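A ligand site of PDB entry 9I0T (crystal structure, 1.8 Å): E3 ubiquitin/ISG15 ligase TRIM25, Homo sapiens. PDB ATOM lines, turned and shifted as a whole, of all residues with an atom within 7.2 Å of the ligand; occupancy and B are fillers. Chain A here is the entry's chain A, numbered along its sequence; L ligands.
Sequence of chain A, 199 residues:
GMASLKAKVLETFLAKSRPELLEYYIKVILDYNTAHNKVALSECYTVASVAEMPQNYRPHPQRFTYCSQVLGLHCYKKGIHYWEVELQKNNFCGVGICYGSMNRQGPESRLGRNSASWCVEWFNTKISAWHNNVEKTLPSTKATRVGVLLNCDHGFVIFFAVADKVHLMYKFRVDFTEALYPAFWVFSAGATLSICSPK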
ATOM      1  N   HIS A  36     -18.456  -0.487  -7.324  1.00  0.00           N
ATOM      2  CA  HIS A  36     -18.908   0.060  -6.053  1.00  0.00           C
ATOM      3  C   HIS A  36     -20.134   0.944  -6.272  1.00  0.00           C
ATOM      4  O   HIS A  36     -20.314   1.534  -7.338  1.00  0.00           O
ATOM      5  CB  HIS A  36     -17.762   0.868  -5.420  1.00  0.00           C
ATOM      6  CG  HIS A  36     -18.041   1.389  -4.042  1.00  0.00           C
ATOM      7  ND1 HIS A  36     -18.609   2.622  -3.815  1.00  0.00           N
ATOM      8  CD2 HIS A  36     -17.746   0.877  -2.820  1.00  0.00           C
ATOM      9  CE1 HIS A  36     -18.698   2.836  -2.514  1.00  0.00           C
ATOM     10  NE2 HIS A  36     -18.174   1.800  -1.885  1.00  0.00           N
ATOM     11  N   LYS A  38     -20.819   3.808  -5.375  1.00  0.00           N
ATOM     12  CA  LYS A  38     -20.550   5.204  -5.693  1.00  0.00           C
ATOM     13  C   LYS A  38     -20.028   5.404  -7.105  1.00  0.00           C
ATOM     14  O   LYS A  38     -19.742   6.540  -7.501  1.00  0.00           O
ATOM     15  CB  LYS A  38     -19.553   5.771  -4.673  1.00  0.00           C
ATOM     16  CG  LYS A  38     -20.184   6.058  -3.303  1.00  0.00           C
ATOM     17  CD  LYS A  38     -21.082   7.295  -3.329  1.00  0.00           C
ATOM     18  CE  LYS A  38     -20.256   8.579  -3.413  1.00  0.00           C
ATOM     19  NZ  LYS A  38     -21.072   9.824  -3.261  1.00  0.00           N
ATOM     20  N   TYR A  66     -15.883  -1.340  -0.321  1.00  0.00           N
ATOM     21  CA  TYR A  66     -15.139  -0.376   0.497  1.00  0.00           C
ATOM     22  C   TYR A  66     -14.554   0.769  -0.307  1.00  0.00           C
ATOM     23  O   TYR A  66     -14.616   1.922   0.132  1.00  0.00           O
ATOM     24  CB  TYR A  66     -14.012  -1.098   1.232  1.00  0.00           C
ATOM     25  CG  TYR A  66     -13.316  -0.264   2.281  1.00  0.00           C
ATOM     26  CD1 TYR A  66     -13.900  -0.035   3.510  1.00  0.00           C
ATOM     27  CD2 TYR A  66     -12.049   0.270   2.040  1.00  0.00           C
ATOM     28  CE1 TYR A  66     -13.260   0.726   4.475  1.00  0.00           C
ATOM     29  CE2 TYR A  66     -11.399   1.032   3.004  1.00  0.00           C
ATOM     30  CZ  TYR A  66     -12.014   1.252   4.214  1.00  0.00           C
ATOM     31  OH  TYR A  66     -11.382   2.002   5.185  1.00  0.00           O
ATOM     32  N   CYS A  67     -13.985   0.496  -1.483  1.00  0.00           N
ATOM     33  CA  CYS A  67     -13.398   1.522  -2.316  1.00  0.00           C
ATOM     34  C   CYS A  67     -14.201   1.679  -3.601  1.00  0.00           C
ATOM     35  O   CYS A  67     -14.714   0.703  -4.152  1.00  0.00           O
ATOM     36  CB  CYS A  67     -11.944   1.192  -2.644  1.00  0.00           C
ATOM     37  SG  CYS A  67     -10.832   1.680  -1.315  1.00  0.00           S
ATOM     38  N   SER A  68     -14.317   2.927  -4.060  1.00  0.00           N
ATOM     39  CA  SER A  68     -15.164   3.272  -5.196  1.00  0.00           C
ATOM     40  C   SER A  68     -14.420   2.932  -6.491  1.00  0.00           C
ATOM     41  O   SER A  68     -13.933   3.803  -7.234  1.00  0.00           O
ATOM     42  CB  SER A  68     -15.611   4.721  -5.124  1.00  0.00           C
ATOM     43  OG  SER A  68     -14.564   5.566  -4.651  1.00  0.00           O
ATOM     44  N   GLN A  69     -14.349   1.638  -6.775  1.00  0.00           N
ATOM     45  CA  GLN A  69     -13.555   1.081  -7.862  1.00  0.00           C
ATOM     46  C   GLN A  69     -14.425   0.223  -8.779  1.00  0.00           C
ATOM     47  O   GLN A  69     -15.570  -0.120  -8.457  1.00  0.00           O
ATOM     48  CB  GLN A  69     -12.376   0.271  -7.295  1.00  0.00           C
ATOM     49  CG  GLN A  69     -11.494   1.129  -6.365  1.00  0.00           C
ATOM     50  CD  GLN A  69     -10.390   0.356  -5.657  1.00  0.00           C
ATOM     51  OE1 GLN A  69      -9.359   0.944  -5.278  1.00  0.00           O
ATOM     52  NE2 GLN A  69     -10.592  -0.937  -5.455  1.00  0.00           N
ATOM     53  N   PHE A  92      -9.652  13.477  -8.115  1.00  0.00           N
ATOM     54  CA  PHE A  92      -9.129  12.299  -7.402  1.00  0.00           C
ATOM     55  C   PHE A  92      -9.581  11.033  -8.130  1.00  0.00           C
ATOM     56  O   PHE A  92     -10.755  10.676  -8.090  1.00  0.00           O
ATOM     57  CB  PHE A  92      -9.667  12.231  -5.972  1.00  0.00           C
ATOM     58  CG  PHE A  92      -9.009  13.154  -4.996  1.00  0.00           C
ATOM     59  CD1 PHE A  92      -9.058  14.531  -5.166  1.00  0.00           C
ATOM     60  CD2 PHE A  92      -8.404  12.638  -3.859  1.00  0.00           C
ATOM     61  CE1 PHE A  92      -8.471  15.376  -4.236  1.00  0.00           C
ATOM     62  CE2 PHE A  92      -7.817  13.489  -2.921  1.00  0.00           C
ATOM     63  CZ  PHE A  92      -7.854  14.849  -3.103  1.00  0.00           C
ATOM     64  N   GLY A 106     -12.947  -4.250   2.325  1.00  0.00           N
ATOM     65  CA  GLY A 106     -11.992  -3.760   3.287  1.00  0.00           C
ATOM     66  C   GLY A 106     -10.902  -2.891   2.682  1.00  0.00           C
ATOM     67  O   GLY A 106     -10.818  -2.703   1.460  1.00  0.00           O
ATOM     68  N   PRO A 107     -10.047  -2.325   3.543  1.00  0.00           N
ATOM     69  CA  PRO A 107      -8.949  -1.477   3.050  1.00  0.00           C
ATOM     70  C   PRO A 107      -7.980  -2.210   2.159  1.00  0.00           C
ATOM     71  O   PRO A 107      -7.305  -1.576   1.352  1.00  0.00           O
ATOM     72  CB  PRO A 107      -8.270  -1.000   4.350  1.00  0.00           C
ATOM     73  CG  PRO A 107      -9.303  -1.172   5.404  1.00  0.00           C
ATOM     74  CD  PRO A 107     -10.088  -2.380   5.014  1.00  0.00           C
ATOM     75  N   SER A 109      -8.705  -3.878  -0.319  1.00  0.00           N
ATOM     76  CA  SER A 109      -9.198  -3.822  -1.686  1.00  0.00           C
ATOM     77  C   SER A 109      -8.718  -2.595  -2.451  1.00  0.00           C
ATOM     78  O   SER A 109      -8.971  -2.511  -3.661  1.00  0.00           O
ATOM     79  CB  SER A 109     -10.738  -3.849  -1.697  1.00  0.00           C
ATOM     80  OG  SER A 109     -11.257  -2.690  -1.106  1.00  0.00           O
ATOM     81  N   ARG A 110      -8.053  -1.647  -1.806  1.00  0.00           N
ATOM     82  CA  ARG A 110      -7.689  -0.403  -2.478  1.00  0.00           C
ATOM     83  C   ARG A 110      -6.541  -0.623  -3.444  1.00  0.00           C
ATOM     84  O   ARG A 110      -5.491  -1.188  -3.083  1.00  0.00           O
ATOM     85  CB  ARG A 110      -7.328   0.675  -1.458  1.00  0.00           C
ATOM     86  CG  ARG A 110      -7.129   2.061  -2.049  1.00  0.00           C
ATOM     87  CD  ARG A 110      -7.002   3.083  -0.937  1.00  0.00           C
ATOM     88  NE  ARG A 110      -6.922   4.455  -1.426  1.00  0.00           N
ATOM     89  CZ  ARG A 110      -6.920   5.507  -0.615  1.00  0.00           C
ATOM     90  NH1 ARG A 110      -6.986   5.380   0.687  1.00  0.00           N
ATOM     91  NH2 ARG A 110      -6.855   6.732  -1.150  1.00  0.00           N
ATOM     92  N   LEU A 111      -6.724  -0.161  -4.678  1.00  0.00           N
ATOM     93  CA  LEU A 111      -5.717  -0.334  -5.716  1.00  0.00           C
ATOM     94  C   LEU A 111      -4.390   0.275  -5.306  1.00  0.00           C
ATOM     95  O   LEU A 111      -4.322   1.417  -4.832  1.00  0.00           O
ATOM     96  CB  LEU A 111      -6.204   0.304  -7.016  1.00  0.00           C
ATOM     97  CG  LEU A 111      -7.342  -0.425  -7.702  1.00  0.00           C
ATOM     98  CD1 LEU A 111      -7.838   0.432  -8.860  1.00  0.00           C
ATOM     99  CD2 LEU A 111      -6.867  -1.788  -8.169  1.00  0.00           C
ATOM    100  N   ARG A 113      -2.516  -0.601  -2.891  1.00  0.00           N
ATOM    101  CA  ARG A 113      -2.211  -0.768  -1.479  1.00  0.00           C
ATOM    102  C   ARG A 113      -2.088  -2.233  -1.103  1.00  0.00           C
ATOM    103  O   ARG A 113      -2.152  -2.584   0.073  1.00  0.00           O
ATOM    104  CB  ARG A 113      -3.269  -0.063  -0.608  1.00  0.00           C
ATOM    105  CG  ARG A 113      -3.036   1.441  -0.422  1.00  0.00           C
ATOM    106  CD  ARG A 113      -3.179   2.216  -1.708  1.00  0.00           C
ATOM    107  NE  ARG A 113      -3.302   3.658  -1.514  1.00  0.00           N
ATOM    108  CZ  ARG A 113      -3.569   4.507  -2.491  1.00  0.00           C
ATOM    109  NH1 ARG A 113      -3.747   4.077  -3.739  1.00  0.00           N
ATOM    110  NH2 ARG A 113      -3.672   5.806  -2.224  1.00  0.00           N
ATOM    111  N   GLU A 121      -2.190   7.257  -9.797  1.00  0.00           N
ATOM    112  CA  GLU A 121      -3.299   7.836  -9.071  1.00  0.00           C
ATOM    113  C   GLU A 121      -3.117   9.341  -8.972  1.00  0.00           C
ATOM    114  O   GLU A 121      -2.011   9.810  -8.691  1.00  0.00           O
ATOM    115  CB  GLU A 121      -3.405   7.214  -7.690  1.00  0.00           C
ATOM    116  CG  GLU A 121      -4.445   7.807  -6.791  1.00  0.00           C
ATOM    117  CD  GLU A 121      -4.533   7.048  -5.510  1.00  0.00           C
ATOM    118  OE1 GLU A 121      -4.837   5.842  -5.574  1.00  0.00           O
ATOM    119  OE2 GLU A 121      -4.265   7.628  -4.446  1.00  0.00           O
ATOM    120  N   TRP A 122      -4.190  10.071  -9.227  1.00  0.00           N
ATOM    121  CA  TRP A 122      -4.250  11.515  -9.021  1.00  0.00           C
ATOM    122  C   TRP A 122      -4.931  11.732  -7.677  1.00  0.00           C
ATOM    123  O   TRP A 122      -6.048  11.247  -7.466  1.00  0.00           O
ATOM    124  CB  TRP A 122      -5.034  12.188 -10.160  1.00  0.00           C
ATOM    125  CG  TRP A 122      -4.342  12.158 -11.508  1.00  0.00           C
ATOM    126  CD1 TRP A 122      -3.737  13.207 -12.150  1.00  0.00           C
ATOM    127  CD2 TRP A 122      -4.190  11.023 -12.379  1.00  0.00           C
ATOM    128  NE1 TRP A 122      -3.237  12.804 -13.360  1.00  0.00           N
ATOM    129  CE2 TRP A 122      -3.494  11.467 -13.528  1.00  0.00           C
ATOM    130  CE3 TRP A 122      -4.583   9.685 -12.308  1.00  0.00           C
ATOM    131  CZ2 TRP A 122      -3.177  10.609 -14.593  1.00  0.00           C
ATOM    132  CZ3 TRP A 122      -4.267   8.832 -13.365  1.00  0.00           C
ATOM    133  CH2 TRP A 122      -3.574   9.306 -14.486  1.00  0.00           C
ATOM    134  N   PHE A 123      -4.251  12.416  -6.769  1.00  0.00           N
ATOM    135  CA  PHE A 123      -4.692  12.499  -5.378  1.00  0.00           C
ATOM    136  C   PHE A 123      -4.231  13.853  -4.854  1.00  0.00           C
ATOM    137  O   PHE A 123      -3.037  14.037  -4.608  1.00  0.00           O
ATOM    138  CB  PHE A 123      -4.101  11.344  -4.570  1.00  0.00           C
ATOM    139  CG  PHE A 123      -4.573  11.264  -3.130  1.00  0.00           C
ATOM    140  CD1 PHE A 123      -4.291  12.268  -2.219  1.00  0.00           C
ATOM    141  CD2 PHE A 123      -5.282  10.163  -2.684  1.00  0.00           C
ATOM    142  CE1 PHE A 123      -4.714  12.180  -0.905  1.00  0.00           C
ATOM    143  CE2 PHE A 123      -5.703  10.061  -1.372  1.00  0.00           C
ATOM    144  CZ  PHE A 123      -5.425  11.076  -0.481  1.00  0.00           C
ATOM    145  N   ASN A 124      -5.174  14.784  -4.687  1.00  0.00           N
ATOM    146  CA  ASN A 124      -4.867  16.125  -4.171  1.00  0.00           C
ATOM    147  C   ASN A 124      -3.949  16.887  -5.131  1.00  0.00           C
ATOM    148  O   ASN A 124      -3.001  17.546  -4.705  1.00  0.00           O
ATOM    149  CB  ASN A 124      -4.244  16.051  -2.778  1.00  0.00           C
ATOM    150  CG  ASN A 124      -5.078  16.764  -1.737  1.00  0.00           C
ATOM    151  OD1 ASN A 124      -6.039  17.458  -2.074  1.00  0.00           O
ATOM    152  ND2 ASN A 124      -4.692  16.626  -0.463  1.00  0.00           N
ATOM    153  N   TRP A 185     -10.376   3.689 -10.293  1.00  0.00           N
ATOM    154  CA  TRP A 185     -10.828   4.316  -9.051  1.00  0.00           C
ATOM    155  C   TRP A 185     -11.303   5.730  -9.366  1.00  0.00           C
ATOM    156  O   TRP A 185     -10.599   6.483 -10.047  1.00  0.00           O
ATOM    157  CB  TRP A 185      -9.696   4.356  -8.022  1.00  0.00           C
ATOM    158  CG  TRP A 185     -10.048   5.038  -6.706  1.00  0.00           C
ATOM    159  CD1 TRP A 185     -11.006   4.669  -5.808  1.00  0.00           C
ATOM    160  CD2 TRP A 185      -9.420   6.208  -6.139  1.00  0.00           C
ATOM    161  NE1 TRP A 185     -11.022   5.524  -4.731  1.00  0.00           N
ATOM    162  CE2 TRP A 185     -10.065   6.479  -4.915  1.00  0.00           C
ATOM    163  CE3 TRP A 185      -8.387   7.059  -6.563  1.00  0.00           C
ATOM    164  CZ2 TRP A 185      -9.696   7.556  -4.099  1.00  0.00           C
ATOM    165  CZ3 TRP A 185      -8.025   8.126  -5.741  1.00  0.00           C
ATOM    166  CH2 TRP A 185      -8.675   8.361  -4.530  1.00  0.00           C
ATOM    167  N   VAL A 186     -12.489   6.100  -8.876  1.00  0.00           N
ATOM    168  CA  VAL A 186     -12.966   7.482  -9.000  1.00  0.00           C
ATOM    169  C   VAL A 186     -13.489   7.931  -7.641  1.00  0.00           C
ATOM    170  O   VAL A 186     -14.194   7.173  -6.968  1.00  0.00           O
ATOM    171  CB  VAL A 186     -14.055   7.644 -10.081  1.00  0.00           C
ATOM    172  CG1 VAL A 186     -13.470   7.464 -11.475  1.00  0.00           C
ATOM    173  CG2 VAL A 186     -15.199   6.674  -9.856  1.00  0.00           C
ATOM    174  N   PHE A 187     -13.125   9.142  -7.229  1.00  0.00           N
ATOM    175  CA  PHE A 187     -13.538   9.595  -5.893  1.00  0.00           C
ATOM    176  C   PHE A 187     -14.065  11.019  -5.842  1.00  0.00           C
ATOM    177  O   PHE A 187     -15.119  11.267  -5.242  1.00  0.00           O
ATOM    178  CB  PHE A 187     -12.389   9.440  -4.901  1.00  0.00           C
ATOM    179  CG  PHE A 187     -12.693  10.013  -3.546  1.00  0.00           C
ATOM    180  CD1 PHE A 187     -13.413   9.273  -2.620  1.00  0.00           C
ATOM    181  CD2 PHE A 187     -12.276  11.279  -3.205  1.00  0.00           C
ATOM    182  CE1 PHE A 187     -13.707   9.795  -1.363  1.00  0.00           C
ATOM    183  CE2 PHE A 187     -12.563  11.816  -1.947  1.00  0.00           C
ATOM    184  CZ  PHE A 187     -13.281  11.062  -1.024  1.00  0.00           C
ATOM    185  N   SER A 188     -13.366  11.989  -6.441  1.00  0.00           N
ATOM    186  CA  SER A 188     -13.826  13.365  -6.343  1.00  0.00           C
ATOM    187  C   SER A 188     -15.101  13.577  -7.161  1.00  0.00           C
ATOM    188  O   SER A 188     -15.402  12.833  -8.103  1.00  0.00           O
ATOM    189  CB  SER A 188     -12.752  14.341  -6.803  1.00  0.00           C
ATOM    190  OG  SER A 188     -12.419  14.106  -8.168  1.00  0.00           O
HETATM  191  C1  LIG L   1     -13.733   6.697   0.098  1.00  0.00           C
HETATM  192  C2  LIG L   1      -8.424  14.782   0.497  1.00  0.00           C
HETATM  193  C3  LIG L   1     -13.279   6.995   1.526  1.00  0.00           C
HETATM  194  C4  LIG L   1     -10.898   6.565   2.074  1.00  0.00           C
HETATM  195  C5  LIG L   1      -9.269  12.116   0.957  1.00  0.00           C
HETATM  196  C6  LIG L   1     -10.495   8.014   1.759  1.00  0.00           C
HETATM  197  C7  LIG L   1     -10.492   9.046   2.885  1.00  0.00           C
HETATM  198  C8  LIG L   1     -10.130  10.285   2.627  1.00  0.00           C
HETATM  199  C9  LIG L   1      -9.699  10.672   1.219  1.00  0.00           C
HETATM  200  C10 LIG L   1      -7.999  12.439   1.135  1.00  0.00           C
HETATM  201  C11 LIG L   1      -7.545  13.877   0.890  1.00  0.00           C
HETATM  202  N1  LIG L   1     -12.706   4.444  -0.105  1.00  0.00           N
HETATM  203  N2  LIG L   1     -12.255   6.070   1.972  1.00  0.00           N
HETATM  204  C12 LIG L   1     -13.933   5.214  -0.199  1.00  0.00           C
HETATM  205  C13 LIG L   1     -10.683   3.486  -1.382  1.00  0.00           C
HETATM  206  C14 LIG L   1      -9.889  14.403   0.303  1.00  0.00           C
HETATM  207  C15 LIG L   1     -10.289  13.173   0.518  1.00  0.00           C
HETATM  208  C16 LIG L   1      -9.683   9.781   0.252  1.00  0.00           C
HETATM  209  C17 LIG L   1      -9.246  10.190  -1.146  1.00  0.00           C
HETATM  210  C18 LIG L   1     -10.102   8.348   0.543  1.00  0.00           C
HETATM  211  C19 LIG L   1     -11.976   4.297  -1.349  1.00  0.00           C
HETATM  212  C20 LIG L   1     -12.396   4.659   2.304  1.00  0.00           C
HETATM  213  C21 LIG L   1     -12.122   3.807   1.065  1.00  0.00           C
HETATM  214  O1  LIG L   1     -12.437   4.801  -2.329  1.00  0.00           O
HETATM  215  O2  LIG L   1     -10.029   5.834   2.434  1.00  0.00           O
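The side-chain sulfur of Cys 67 is covalently linked to a carbon (C13) of the ligand, 1.8 Å away.
NE1 of Trp 185 lies within hydrogen-bond range of O1 of the ligand.
The backbone NH (N) of Ser 68 lies within hydrogen-bond range of an oxygen (O1) of the ligand, 3.2 Å away.
The side-chain hydroxyl (OG) of Ser 68 sits at hydrogen-bond distance from an oxygen (O1) of the ligand (3.2 Å).
The backbone carbonyl oxygen (O) of Val 186 is in hydrogen-bond range of the side-chain hydroxyl (OG) of Ser 68.
O of Phe 92 sits at hydrogen-bond distance from N of Phe 187 (3.0 Å).
OG of Ser 188 lies within hydrogen-bond range of N of Phe 92, at 2.8 Å.
The backbone carbonyl oxygen (O) of Tyr 66 lies close to a nitrogen (N1) of the ligand (3.2 Å).
Phe 92 touches the ligand (CZ to C2, 3.6 Å).
Arg 110 touches the ligand.
Phe 123 touches the ligand (CZ to C10, 3.3 Å).
Phe 187 touches the ligand (CE1 to C1, 3.4 Å).
The nearest printed residue that does not touch the ligand is Asn 124 (4.2 Å).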
